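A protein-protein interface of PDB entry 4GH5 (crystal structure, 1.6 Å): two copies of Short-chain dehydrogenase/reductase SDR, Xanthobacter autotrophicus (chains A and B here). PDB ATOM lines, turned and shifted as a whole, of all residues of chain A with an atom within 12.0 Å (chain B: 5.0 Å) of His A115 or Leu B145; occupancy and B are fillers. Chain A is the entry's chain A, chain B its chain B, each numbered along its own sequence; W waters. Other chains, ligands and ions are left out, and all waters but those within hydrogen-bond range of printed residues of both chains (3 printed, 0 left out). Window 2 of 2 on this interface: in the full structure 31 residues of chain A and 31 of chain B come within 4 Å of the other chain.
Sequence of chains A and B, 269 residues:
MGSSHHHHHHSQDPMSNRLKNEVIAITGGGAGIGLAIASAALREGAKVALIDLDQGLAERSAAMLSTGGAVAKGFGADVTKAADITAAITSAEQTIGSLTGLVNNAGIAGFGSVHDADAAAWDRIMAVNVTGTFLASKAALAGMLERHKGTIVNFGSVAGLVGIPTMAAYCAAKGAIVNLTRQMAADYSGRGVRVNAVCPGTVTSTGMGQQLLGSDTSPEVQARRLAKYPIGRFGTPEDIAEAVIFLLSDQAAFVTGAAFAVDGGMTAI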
ATOM      1  N   PHE A 111     -11.943  24.870 -25.661  1.00  0.00           N
ATOM      2  CA  PHE A 111     -12.133  24.511 -24.267  1.00  0.00           C
ATOM      3  C   PHE A 111     -13.320  25.229 -23.668  1.00  0.00           C
ATOM      4  O   PHE A 111     -13.726  26.298 -24.134  1.00  0.00           O
ATOM      5  CB  PHE A 111     -10.883  24.855 -23.466  1.00  0.00           C
ATOM      6  CG  PHE A 111      -9.669  24.078 -23.876  1.00  0.00           C
ATOM      7  CD1 PHE A 111      -9.506  22.763 -23.476  1.00  0.00           C
ATOM      8  CD2 PHE A 111      -8.686  24.663 -24.662  1.00  0.00           C
ATOM      9  CE1 PHE A 111      -8.388  22.043 -23.849  1.00  0.00           C
ATOM     10  CE2 PHE A 111      -7.565  23.949 -25.033  1.00  0.00           C
ATOM     11  CZ  PHE A 111      -7.415  22.638 -24.628  1.00  0.00           C
ATOM     12  N   GLY A 112     -13.855  24.647 -22.600  1.00  0.00           N
ATOM     13  CA  GLY A 112     -15.023  25.185 -21.939  1.00  0.00           C
ATOM     14  C   GLY A 112     -15.874  24.044 -21.426  1.00  0.00           C
ATOM     15  O   GLY A 112     -16.196  23.129 -22.174  1.00  0.00           O
ATOM     16  N   SER A 113     -16.232  24.108 -20.150  1.00  0.00           N
ATOM     17  CA  SER A 113     -17.092  23.106 -19.539  1.00  0.00           C
ATOM     18  C   SER A 113     -18.526  23.610 -19.611  1.00  0.00           C
ATOM     19  O   SER A 113     -18.753  24.772 -19.929  1.00  0.00           O
ATOM     20  CB  SER A 113     -16.680  22.889 -18.084  1.00  0.00           C
ATOM     21  OG  SER A 113     -15.368  22.361 -17.998  1.00  0.00           O
ATOM     22  N   VAL A 114     -19.504  22.767 -19.306  1.00  0.00           N
ATOM     23  CA  VAL A 114     -20.893  23.220 -19.352  1.00  0.00           C
ATOM     24  C   VAL A 114     -21.126  24.483 -18.513  1.00  0.00           C
ATOM     25  O   VAL A 114     -21.877  25.371 -18.923  1.00  0.00           O
ATOM     26  CB  VAL A 114     -21.851  22.111 -18.926  1.00  0.00           C
ATOM     27  N   HIS A 115     -20.466  24.587 -17.361  1.00  0.00           N
ATOM     28  CA  HIS A 115     -20.788  25.691 -16.457  1.00  0.00           C
ATOM     29  C   HIS A 115     -20.209  27.030 -16.897  1.00  0.00           C
ATOM     30  O   HIS A 115     -20.719  28.075 -16.488  1.00  0.00           O
ATOM     31  CB  HIS A 115     -20.375  25.390 -15.002  1.00  0.00           C
ATOM     32  CG  HIS A 115     -18.906  25.524 -14.746  1.00  0.00           C
ATOM     33  ND1 HIS A 115     -17.994  24.561 -15.120  1.00  0.00           N
ATOM     34  CD2 HIS A 115     -18.188  26.505 -14.145  1.00  0.00           C
ATOM     35  CE1 HIS A 115     -16.780  24.943 -14.767  1.00  0.00           C
ATOM     36  NE2 HIS A 115     -16.870  26.119 -14.171  1.00  0.00           N
ATOM     37  N   ASP A 116     -19.167  27.005 -17.731  1.00  0.00           N
ATOM     38  CA  ASP A 116     -18.477  28.250 -18.070  1.00  0.00           C
ATOM     39  C   ASP A 116     -18.218  28.464 -19.558  1.00  0.00           C
ATOM     40  O   ASP A 116     -17.616  29.468 -19.932  1.00  0.00           O
ATOM     41  CB  ASP A 116     -17.161  28.371 -17.281  1.00  0.00           C
ATOM     42  CG  ASP A 116     -16.146  27.295 -17.643  1.00  0.00           C
ATOM     43  OD1 ASP A 116     -16.487  26.375 -18.407  1.00  0.00           O
ATOM     44  OD2 ASP A 116     -15.000  27.360 -17.142  1.00  0.00           O
ATOM     45  N   ALA A 117     -18.671  27.548 -20.410  1.00  0.00           N
ATOM     46  CA  ALA A 117     -18.368  27.670 -21.835  1.00  0.00           C
ATOM     47  C   ALA A 117     -19.084  28.864 -22.450  1.00  0.00           C
ATOM     48  O   ALA A 117     -20.225  29.169 -22.095  1.00  0.00           O
ATOM     49  CB  ALA A 117     -18.763  26.396 -22.588  1.00  0.00           C
ATOM     50  N   ASP A 118     -18.427  29.521 -23.396  1.00  0.00           N
ATOM     51  CA  ASP A 118     -19.111  30.583 -24.108  1.00  0.00           C
ATOM     52  C   ASP A 118     -20.051  30.010 -25.152  1.00  0.00           C
ATOM     53  O   ASP A 118     -19.638  29.198 -25.975  1.00  0.00           O
ATOM     54  CB  ASP A 118     -18.148  31.536 -24.779  1.00  0.00           C
ATOM     55  CG  ASP A 118     -18.878  32.579 -25.587  1.00  0.00           C
ATOM     56  OD1 ASP A 118     -19.518  33.470 -24.978  1.00  0.00           O
ATOM     57  OD2 ASP A 118     -18.837  32.485 -26.817  1.00  0.00           O
ATOM     58  N   ALA A 119     -21.301  30.457 -25.107  1.00  0.00           N
ATOM     59  CA  ALA A 119     -22.358  29.957 -25.977  1.00  0.00           C
ATOM     60  C   ALA A 119     -22.050  30.152 -27.460  1.00  0.00           C
ATOM     61  O   ALA A 119     -22.407  29.317 -28.282  1.00  0.00           O
ATOM     62  CB  ALA A 119     -23.689  30.596 -25.613  1.00  0.00           C
ATOM     63  N   ALA A 120     -21.396  31.259 -27.808  1.00  0.00           N
ATOM     64  CA  ALA A 120     -21.026  31.479 -29.208  1.00  0.00           C
ATOM     65  C   ALA A 120     -19.937  30.515 -29.659  1.00  0.00           C
ATOM     66  O   ALA A 120     -20.004  29.978 -30.763  1.00  0.00           O
ATOM     67  CB  ALA A 120     -20.587  32.933 -29.440  1.00  0.00           C
ATOM     68  N   ALA A 121     -18.934  30.298 -28.809  1.00  0.00           N
ATOM     69  CA  ALA A 121     -17.886  29.324 -29.110  1.00  0.00           C
ATOM     70  C   ALA A 121     -18.481  27.922 -29.230  1.00  0.00           C
ATOM     71  O   ALA A 121     -18.082  27.149 -30.101  1.00  0.00           O
ATOM     72  CB  ALA A 121     -16.795  29.346 -28.060  1.00  0.00           C
ATOM     73  N   TRP A 122     -19.438  27.614 -28.356  1.00  0.00           N
ATOM     74  CA  TRP A 122     -20.143  26.328 -28.385  1.00  0.00           C
ATOM     75  C   TRP A 122     -20.778  26.145 -29.760  1.00  0.00           C
ATOM     76  O   TRP A 122     -20.570  25.123 -30.431  1.00  0.00           O
ATOM     77  CB  TRP A 122     -21.232  26.291 -27.299  1.00  0.00           C
ATOM     78  CG  TRP A 122     -22.023  25.012 -27.265  1.00  0.00           C
ATOM     79  CD1 TRP A 122     -22.968  24.600 -28.163  1.00  0.00           C
ATOM     80  CD2 TRP A 122     -21.930  23.980 -26.280  1.00  0.00           C
ATOM     81  NE1 TRP A 122     -23.462  23.369 -27.802  1.00  0.00           N
ATOM     82  CE2 TRP A 122     -22.850  22.970 -26.644  1.00  0.00           C
ATOM     83  CE3 TRP A 122     -21.172  23.818 -25.114  1.00  0.00           C
ATOM     84  CZ2 TRP A 122     -23.013  21.801 -25.893  1.00  0.00           C
ATOM     85  CZ3 TRP A 122     -21.343  22.668 -24.366  1.00  0.00           C
ATOM     86  CH2 TRP A 122     -22.253  21.673 -24.761  1.00  0.00           C
ATOM     87  N   ILE A 164     -13.989  14.074 -22.224  1.00  0.00           N
ATOM     88  CA  ILE A 164     -12.688  14.704 -22.035  1.00  0.00           C
ATOM     89  C   ILE A 164     -12.868  15.938 -21.175  1.00  0.00           C
ATOM     90  O   ILE A 164     -13.654  16.814 -21.524  1.00  0.00           O
ATOM     91  CB  ILE A 164     -12.081  15.152 -23.389  1.00  0.00           C
ATOM     92  CG1 ILE A 164     -12.002  13.983 -24.376  1.00  0.00           C
ATOM     93  CG2 ILE A 164     -10.713  15.823 -23.170  1.00  0.00           C
ATOM     94  CD1 ILE A 164     -11.078  12.859 -23.946  1.00  0.00           C
ATOM     95  N   PRO A 165     -12.139  16.023 -20.052  1.00  0.00           N
ATOM     96  CA  PRO A 165     -12.278  17.191 -19.176  1.00  0.00           C
ATOM     97  C   PRO A 165     -12.148  18.508 -19.937  1.00  0.00           C
ATOM     98  O   PRO A 165     -11.279  18.629 -20.807  1.00  0.00           O
ATOM     99  CB  PRO A 165     -11.095  17.038 -18.213  1.00  0.00           C
ATOM    100  CG  PRO A 165     -10.915  15.556 -18.106  1.00  0.00           C
ATOM    101  CD  PRO A 165     -11.196  15.031 -19.505  1.00  0.00           C
ATOM    102  N   THR A 166     -13.034  19.448 -19.621  1.00  0.00           N
ATOM    103  CA  THR A 166     -12.998  20.829 -20.105  1.00  0.00           C
ATOM    104  C   THR A 166     -13.245  20.994 -21.607  1.00  0.00           C
ATOM    105  O   THR A 166     -12.906  22.025 -22.171  1.00  0.00           O
ATOM    106  CB  THR A 166     -11.673  21.551 -19.718  1.00  0.00           C
ATOM    107  OG1 THR A 166     -10.622  21.144 -20.603  1.00  0.00           O
ATOM    108  CG2 THR A 166     -11.274  21.221 -18.291  1.00  0.00           C
ATOM    109  N   MET A 167     -13.852  19.996 -22.246  1.00  0.00           N
ATOM    110  CA  MET A 167     -14.165  20.110 -23.675  1.00  0.00           C
ATOM    111  C   MET A 167     -15.608  19.729 -23.972  1.00  0.00           C
ATOM    112  O   MET A 167     -15.874  18.792 -24.732  1.00  0.00           O
ATOM    113  CB  MET A 167     -13.217  19.255 -24.522  1.00  0.00           C
ATOM    114  CG  MET A 167     -11.740  19.584 -24.332  1.00  0.00           C
ATOM    115  SD  MET A 167     -10.712  18.715 -25.534  1.00  0.00           S
ATOM    116  CE  MET A 167     -10.966  19.723 -26.996  1.00  0.00           C
ATOM    117  N   ALA A 168     -16.543  20.453 -23.374  1.00  0.00           N
ATOM    118  CA  ALA A 168     -17.955  20.112 -23.499  1.00  0.00           C
ATOM    119  C   ALA A 168     -18.505  20.185 -24.933  1.00  0.00           C
ATOM    120  O   ALA A 168     -19.072  19.205 -25.435  1.00  0.00           O
ATOM    121  CB  ALA A 168     -18.799  20.970 -22.539  1.00  0.00           C
ATOM    122  N   ALA A 169     -18.341  21.328 -25.604  1.00  0.00           N
ATOM    123  CA  ALA A 169     -18.883  21.451 -26.954  1.00  0.00           C
ATOM    124  C   ALA A 169     -18.251  20.453 -27.930  1.00  0.00           C
ATOM    125  O   ALA A 169     -18.943  19.869 -28.772  1.00  0.00           O
ATOM    126  CB  ALA A 169     -18.729  22.881 -27.464  1.00  0.00           C
ATOM    127  N   TYR A 170     -16.945  20.259 -27.802  1.00  0.00           N
ATOM    128  CA  TYR A 170     -16.204  19.386 -28.703  1.00  0.00           C
ATOM    129  C   TYR A 170     -16.630  17.930 -28.506  1.00  0.00           C
ATOM    130  O   TYR A 170     -16.812  17.197 -29.476  1.00  0.00           O
ATOM    131  CB  TYR A 170     -14.702  19.567 -28.479  1.00  0.00           C
ATOM    132  CG  TYR A 170     -13.838  18.828 -29.474  1.00  0.00           C
ATOM    133  CD1 TYR A 170     -13.780  19.221 -30.812  1.00  0.00           C
ATOM    134  CD2 TYR A 170     -13.087  17.731 -29.077  1.00  0.00           C
ATOM    135  CE1 TYR A 170     -12.984  18.540 -31.726  1.00  0.00           C
ATOM    136  CE2 TYR A 170     -12.296  17.051 -29.969  1.00  0.00           C
ATOM    137  CZ  TYR A 170     -12.241  17.453 -31.284  1.00  0.00           C
ATOM    138  OH  TYR A 170     -11.436  16.761 -32.149  1.00  0.00           O
ATOM    139  N   LYS B 138     -25.912  24.702 -17.538  1.00  0.00           N
ATOM    140  CA  LYS B 138     -25.042  25.816 -17.183  1.00  0.00           C
ATOM    141  C   LYS B 138     -25.663  26.663 -16.068  1.00  0.00           C
ATOM    142  O   LYS B 138     -24.990  27.048 -15.104  1.00  0.00           O
ATOM    143  CB  LYS B 138     -24.775  26.675 -18.413  1.00  0.00           C
ATOM    144  CG  LYS B 138     -23.912  27.891 -18.133  1.00  0.00           C
ATOM    145  CD  LYS B 138     -23.503  28.549 -19.442  1.00  0.00           C
ATOM    146  CE  LYS B 138     -22.624  29.774 -19.192  1.00  0.00           C
ATOM    147  NZ  LYS B 138     -22.272  30.474 -20.463  1.00  0.00           N
ATOM    148  N   LEU B 141     -25.733  24.565 -12.770  1.00  0.00           N
ATOM    149  CA  LEU B 141     -24.427  24.155 -12.245  1.00  0.00           C
ATOM    150  C   LEU B 141     -23.802  25.175 -11.306  1.00  0.00           C
ATOM    151  O   LEU B 141     -23.036  24.807 -10.431  1.00  0.00           O
ATOM    152  CB  LEU B 141     -23.459  23.805 -13.385  1.00  0.00           C
ATOM    153  CG  LEU B 141     -23.640  22.390 -13.956  1.00  0.00           C
ATOM    154  CD1 LEU B 141     -22.981  22.250 -15.313  1.00  0.00           C
ATOM    155  CD2 LEU B 141     -23.076  21.340 -13.006  1.00  0.00           C
ATOM    156  N   ALA B 142     -24.126  26.455 -11.478  1.00  0.00           N
ATOM    157  CA  ALA B 142     -23.563  27.471 -10.589  1.00  0.00           C
ATOM    158  C   ALA B 142     -23.875  27.122  -9.132  1.00  0.00           C
ATOM    159  O   ALA B 142     -22.977  26.992  -8.304  1.00  0.00           O
ATOM    160  CB  ALA B 142     -24.120  28.851 -10.943  1.00  0.00           C
ATOM    161  N   GLY B 143     -25.156  26.914  -8.852  1.00  0.00           N
ATOM    162  CA  GLY B 143     -25.595  26.549  -7.512  1.00  0.00           C
ATOM    163  C   GLY B 143     -25.157  25.159  -7.084  1.00  0.00           C
ATOM    164  O   GLY B 143     -24.705  24.962  -5.958  1.00  0.00           O
ATOM    165  N   MET B 144     -25.288  24.188  -7.979  1.00  0.00           N
ATOM    166  CA  MET B 144     -24.920  22.823  -7.616  1.00  0.00           C
ATOM    167  C   MET B 144     -23.435  22.691  -7.276  1.00  0.00           C
ATOM    168  O   MET B 144     -23.082  22.006  -6.315  1.00  0.00           O
ATOM    169  CB  MET B 144     -25.298  21.845  -8.718  1.00  0.00           C
ATOM    170  CG  MET B 144     -26.794  21.565  -8.812  1.00  0.00           C
ATOM    171  SD  MET B 144     -27.092  20.547 -10.264  1.00  0.00           S
ATOM    172  CE  MET B 144     -28.862  20.319 -10.163  1.00  0.00           C
ATOM    173  N   LEU B 145     -22.577  23.342  -8.056  1.00  0.00           N
ATOM    174  CA  LEU B 145     -21.143  23.309  -7.777  1.00  0.00           C
ATOM    175  C   LEU B 145     -20.810  24.063  -6.497  1.00  0.00           C
ATOM    176  O   LEU B 145     -19.948  23.630  -5.725  1.00  0.00           O
ATOM    177  CB  LEU B 145     -20.346  23.863  -8.954  1.00  0.00           C
ATOM    178  CG  LEU B 145     -20.430  23.014 -10.224  1.00  0.00           C
ATOM    179  CD1 LEU B 145     -19.831  23.769 -11.391  1.00  0.00           C
ATOM    180  CD2 LEU B 145     -19.735  21.667 -10.021  1.00  0.00           C
ATOM    181  N   GLU B 146     -21.497  25.183  -6.270  1.00  0.00           N
ATOM    182  CA  GLU B 146     -21.297  25.955  -5.043  1.00  0.00           C
ATOM    183  C   GLU B 146     -21.617  25.108  -3.807  1.00  0.00           C
ATOM    184  O   GLU B 146     -20.965  25.235  -2.774  1.00  0.00           O
ATOM    185  CB  GLU B 146     -22.139  27.240  -5.051  1.00  0.00           C
ATOM    186  CG  GLU B 146     -21.895  28.132  -3.834  1.00  0.00           C
ATOM    187  CD  GLU B 146     -22.753  29.393  -3.838  1.00  0.00           C
ATOM    188  OE1 GLU B 146     -22.900  30.026  -4.909  1.00  0.00           O
ATOM    189  OE2 GLU B 146     -23.278  29.754  -2.763  1.00  0.00           O
ATOM    190  N   ARG B 147     -22.606  24.225  -3.935  1.00  0.00           N
ATOM    191  CA  ARG B 147     -23.051  23.373  -2.835  1.00  0.00           C
ATOM    192  C   ARG B 147     -22.399  21.985  -2.847  1.00  0.00           C
ATOM    193  O   ARG B 147     -22.639  21.167  -1.955  1.00  0.00           O
ATOM    194  CB  ARG B 147     -24.572  23.235  -2.885  1.00  0.00           C
ATOM    195  CG  ARG B 147     -25.293  24.566  -2.710  1.00  0.00           C
ATOM    196  CD  ARG B 147     -26.795  24.393  -2.634  1.00  0.00           C
ATOM    197  NE  ARG B 147     -27.382  24.024  -3.921  1.00  0.00           N
ATOM    198  CZ  ARG B 147     -27.701  24.893  -4.878  1.00  0.00           C
ATOM    199  NH1 ARG B 147     -27.466  26.194  -4.720  1.00  0.00           N
ATOM    200  NH2 ARG B 147     -28.240  24.456  -6.013  1.00  0.00           N
ATOM    201  N   HIS B 148     -21.566  21.738  -3.852  1.00  0.00           N
ATOM    202  CA  HIS B 148     -20.951  20.422  -4.056  1.00  0.00           C
ATOM    203  C   HIS B 148     -21.974  19.287  -4.014  1.00  0.00           C
ATOM    204  O   HIS B 148     -21.718  18.211  -3.457  1.00  0.00           O
ATOM    205  CB  HIS B 148     -19.828  20.178  -3.042  1.00  0.00           C
ATOM    206  CG  HIS B 148     -18.720  21.181  -3.130  1.00  0.00           C
ATOM    207  ND1 HIS B 148     -17.539  20.930  -3.797  1.00  0.00           N
ATOM    208  CD2 HIS B 148     -18.623  22.443  -2.653  1.00  0.00           C
ATOM    209  CE1 HIS B 148     -16.758  21.995  -3.718  1.00  0.00           C
ATOM    210  NE2 HIS B 148     -17.394  22.927  -3.032  1.00  0.00           N
ATOM    211  N   TYR B 188     -17.465  16.878 -13.467  1.00  0.00           N
ATOM    212  CA  TYR B 188     -18.224  17.261 -12.274  1.00  0.00           C
ATOM    213  C   TYR B 188     -18.459  16.179 -11.220  1.00  0.00           C
ATOM    214  O   TYR B 188     -18.871  16.496 -10.093  1.00  0.00           O
ATOM    215  CB  TYR B 188     -19.572  17.885 -12.679  1.00  0.00           C
ATOM    216  CG  TYR B 188     -19.443  19.091 -13.592  1.00  0.00           C
ATOM    217  CD1 TYR B 188     -18.625  20.167 -13.254  1.00  0.00           C
ATOM    218  CD2 TYR B 188     -20.135  19.148 -14.801  1.00  0.00           C
ATOM    219  CE1 TYR B 188     -18.511  21.277 -14.099  1.00  0.00           C
ATOM    220  CE2 TYR B 188     -20.030  20.244 -15.636  1.00  0.00           C
ATOM    221  CZ  TYR B 188     -19.217  21.301 -15.283  1.00  0.00           C
ATOM    222  OH  TYR B 188     -19.121  22.388 -16.120  1.00  0.00           O
ATOM    223  N   ARG B 191     -16.742  16.717  -8.115  1.00  0.00           N
ATOM    224  CA  ARG B 191     -17.169  17.959  -7.480  1.00  0.00           C
ATOM    225  C   ARG B 191     -18.569  17.858  -6.870  1.00  0.00           C
ATOM    226  O   ARG B 191     -19.150  18.866  -6.469  1.00  0.00           O
ATOM    227  CB  ARG B 191     -17.100  19.111  -8.486  1.00  0.00           C
ATOM    228  CG  ARG B 191     -15.692  19.287  -9.076  1.00  0.00           C
ATOM    229  CD  ARG B 191     -15.583  20.479 -10.022  1.00  0.00           C
ATOM    230  NE  ARG B 191     -15.837  21.755  -9.353  1.00  0.00           N
ATOM    231  CZ  ARG B 191     -15.865  22.925  -9.986  1.00  0.00           C
ATOM    232  NH1 ARG B 191     -15.652  22.971 -11.296  1.00  0.00           N
ATOM    233  NH2 ARG B 191     -16.107  24.047  -9.318  1.00  0.00           N
ATOM    234  N   VAL B 193     -21.369  16.463  -8.344  1.00  0.00           N
ATOM    235  CA  VAL B 193     -22.510  16.494  -9.261  1.00  0.00           C
ATOM    236  C   VAL B 193     -22.461  15.299 -10.217  1.00  0.00           C
ATOM    237  O   VAL B 193     -21.579  15.218 -11.073  1.00  0.00           O
ATOM    238  CB  VAL B 193     -22.572  17.817 -10.062  1.00  0.00           C
ATOM    239  CG1 VAL B 193     -23.813  17.829 -10.940  1.00  0.00           C
ATOM    240  CG2 VAL B 193     -22.595  19.014  -9.104  1.00  0.00           C
HETATM  241  O   HOH W   1     -22.591  28.439 -14.564  1.00  0.00           O
HETATM  242  O   HOH W   2     -16.660  26.409 -10.815  1.00  0.00           O
HETATM  243  O   HOH W   3     -22.080  32.111 -22.921  1.00  0.00           O
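Water W1 lies within hydrogen-bond range of O of His A115 (2.7 Å) and O of Lys B138 (2.8 Å).
Water W3 lies within hydrogen-bond range of the backbone NH of Ala A119 (2.8 Å) and the side-chain amino group of Lys B138 (3.0 Å).
Water W2 lies within hydrogen-bond range of the guanidinium group (NH2) of Arg B191 (2.9 Å) and a ring nitrogen (NE2) of His A115 (3.4 Å).
Among the printed residues, pairs that only touch across the chains: Ser A113 with Tyr B188 (3.2 Å), Val A114 with Lys B138 (3.2 Å), Val A114 with Leu B141 (3.8 Å), His A115 with Lys B138 (3.6 Å), His A115 with Leu B141 (3.8 Å) and His A115 with Leu B145 (3.9 Å).
No position is printed for both chains.
The side-chain carboxylate of Asp A116 lies within hydrogen-bond range of the backbone NH of Ser A113 (2.9 Å).
The backbone carbonyl oxygen (O) of Tyr B188 sits at hydrogen-bond distance from the backbone NH (N) of Val B193, at 3.0 Å.
Printed residues of chain A within 4 Å of Leu B145: His A115 (3.9 Å).
Of chain A, only Val A114 (3.2 Å), His A115 (3.6 Å) and Ala A117 (2.9 Å) come within 4 Å of Lys B138.
Ala B142 touches none of the printed residues of chain A.
No residue of chain A comes within 4 Å of Gly B143.
No residue of chain A comes within 4 Å of Met B144.
No residue of chain A comes within 4 Å of Arg B147.
Tyr B188 touches three residues of chain A.
No residue of chain A comes within 4 Å of Arg B191.
No residue of chain A comes within 4 Å of Val B193.
Printed residues of chain B within 4 Å of Val A114: Lys B138, Leu B141 and Tyr B188.
Printed residues of chain B within 4 Å of Ala A117: Lys B138 (2.9 Å).
Of the printed residues of chain B, Ser A113 touches Tyr B188.
Ala A169 touches none of the printed residues of chain B.
Ala A168 touches none of the printed residues of chain B.
The nearest printed residue of chain B that does not touch Val A114 is Leu B145 (7.3 Å).
The backbone NH of Val A114 is in hydrogen-bond range of the side-chain hydroxyl of Tyr B188 (3.2 Å).
A ring nitrogen (ND1) of His A115 sits at hydrogen-bond distance from the side-chain hydroxyl of Tyr B188.
NZ of Lys B138 sits at hydrogen-bond distance from O of Ala A117, at 2.9 Å.
Along chain A the printed residues that touch a printed residue of chain B span positions 113 to 117.
Of the 12 printed residues of chain B, 4 touch a printed residue of chain A.
Hydrophobic or aromatic side chains of chain B within 4 Å of the printed part of chain A: Leu B141, Leu B145 and Tyr B188.
Among the printed residues, 9 pairs touch across the chains.
Among the printed residues, no Asp or Glu carboxylate lies within 4 Å of a Lys or Arg side-chain nitrogen of the other chain.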
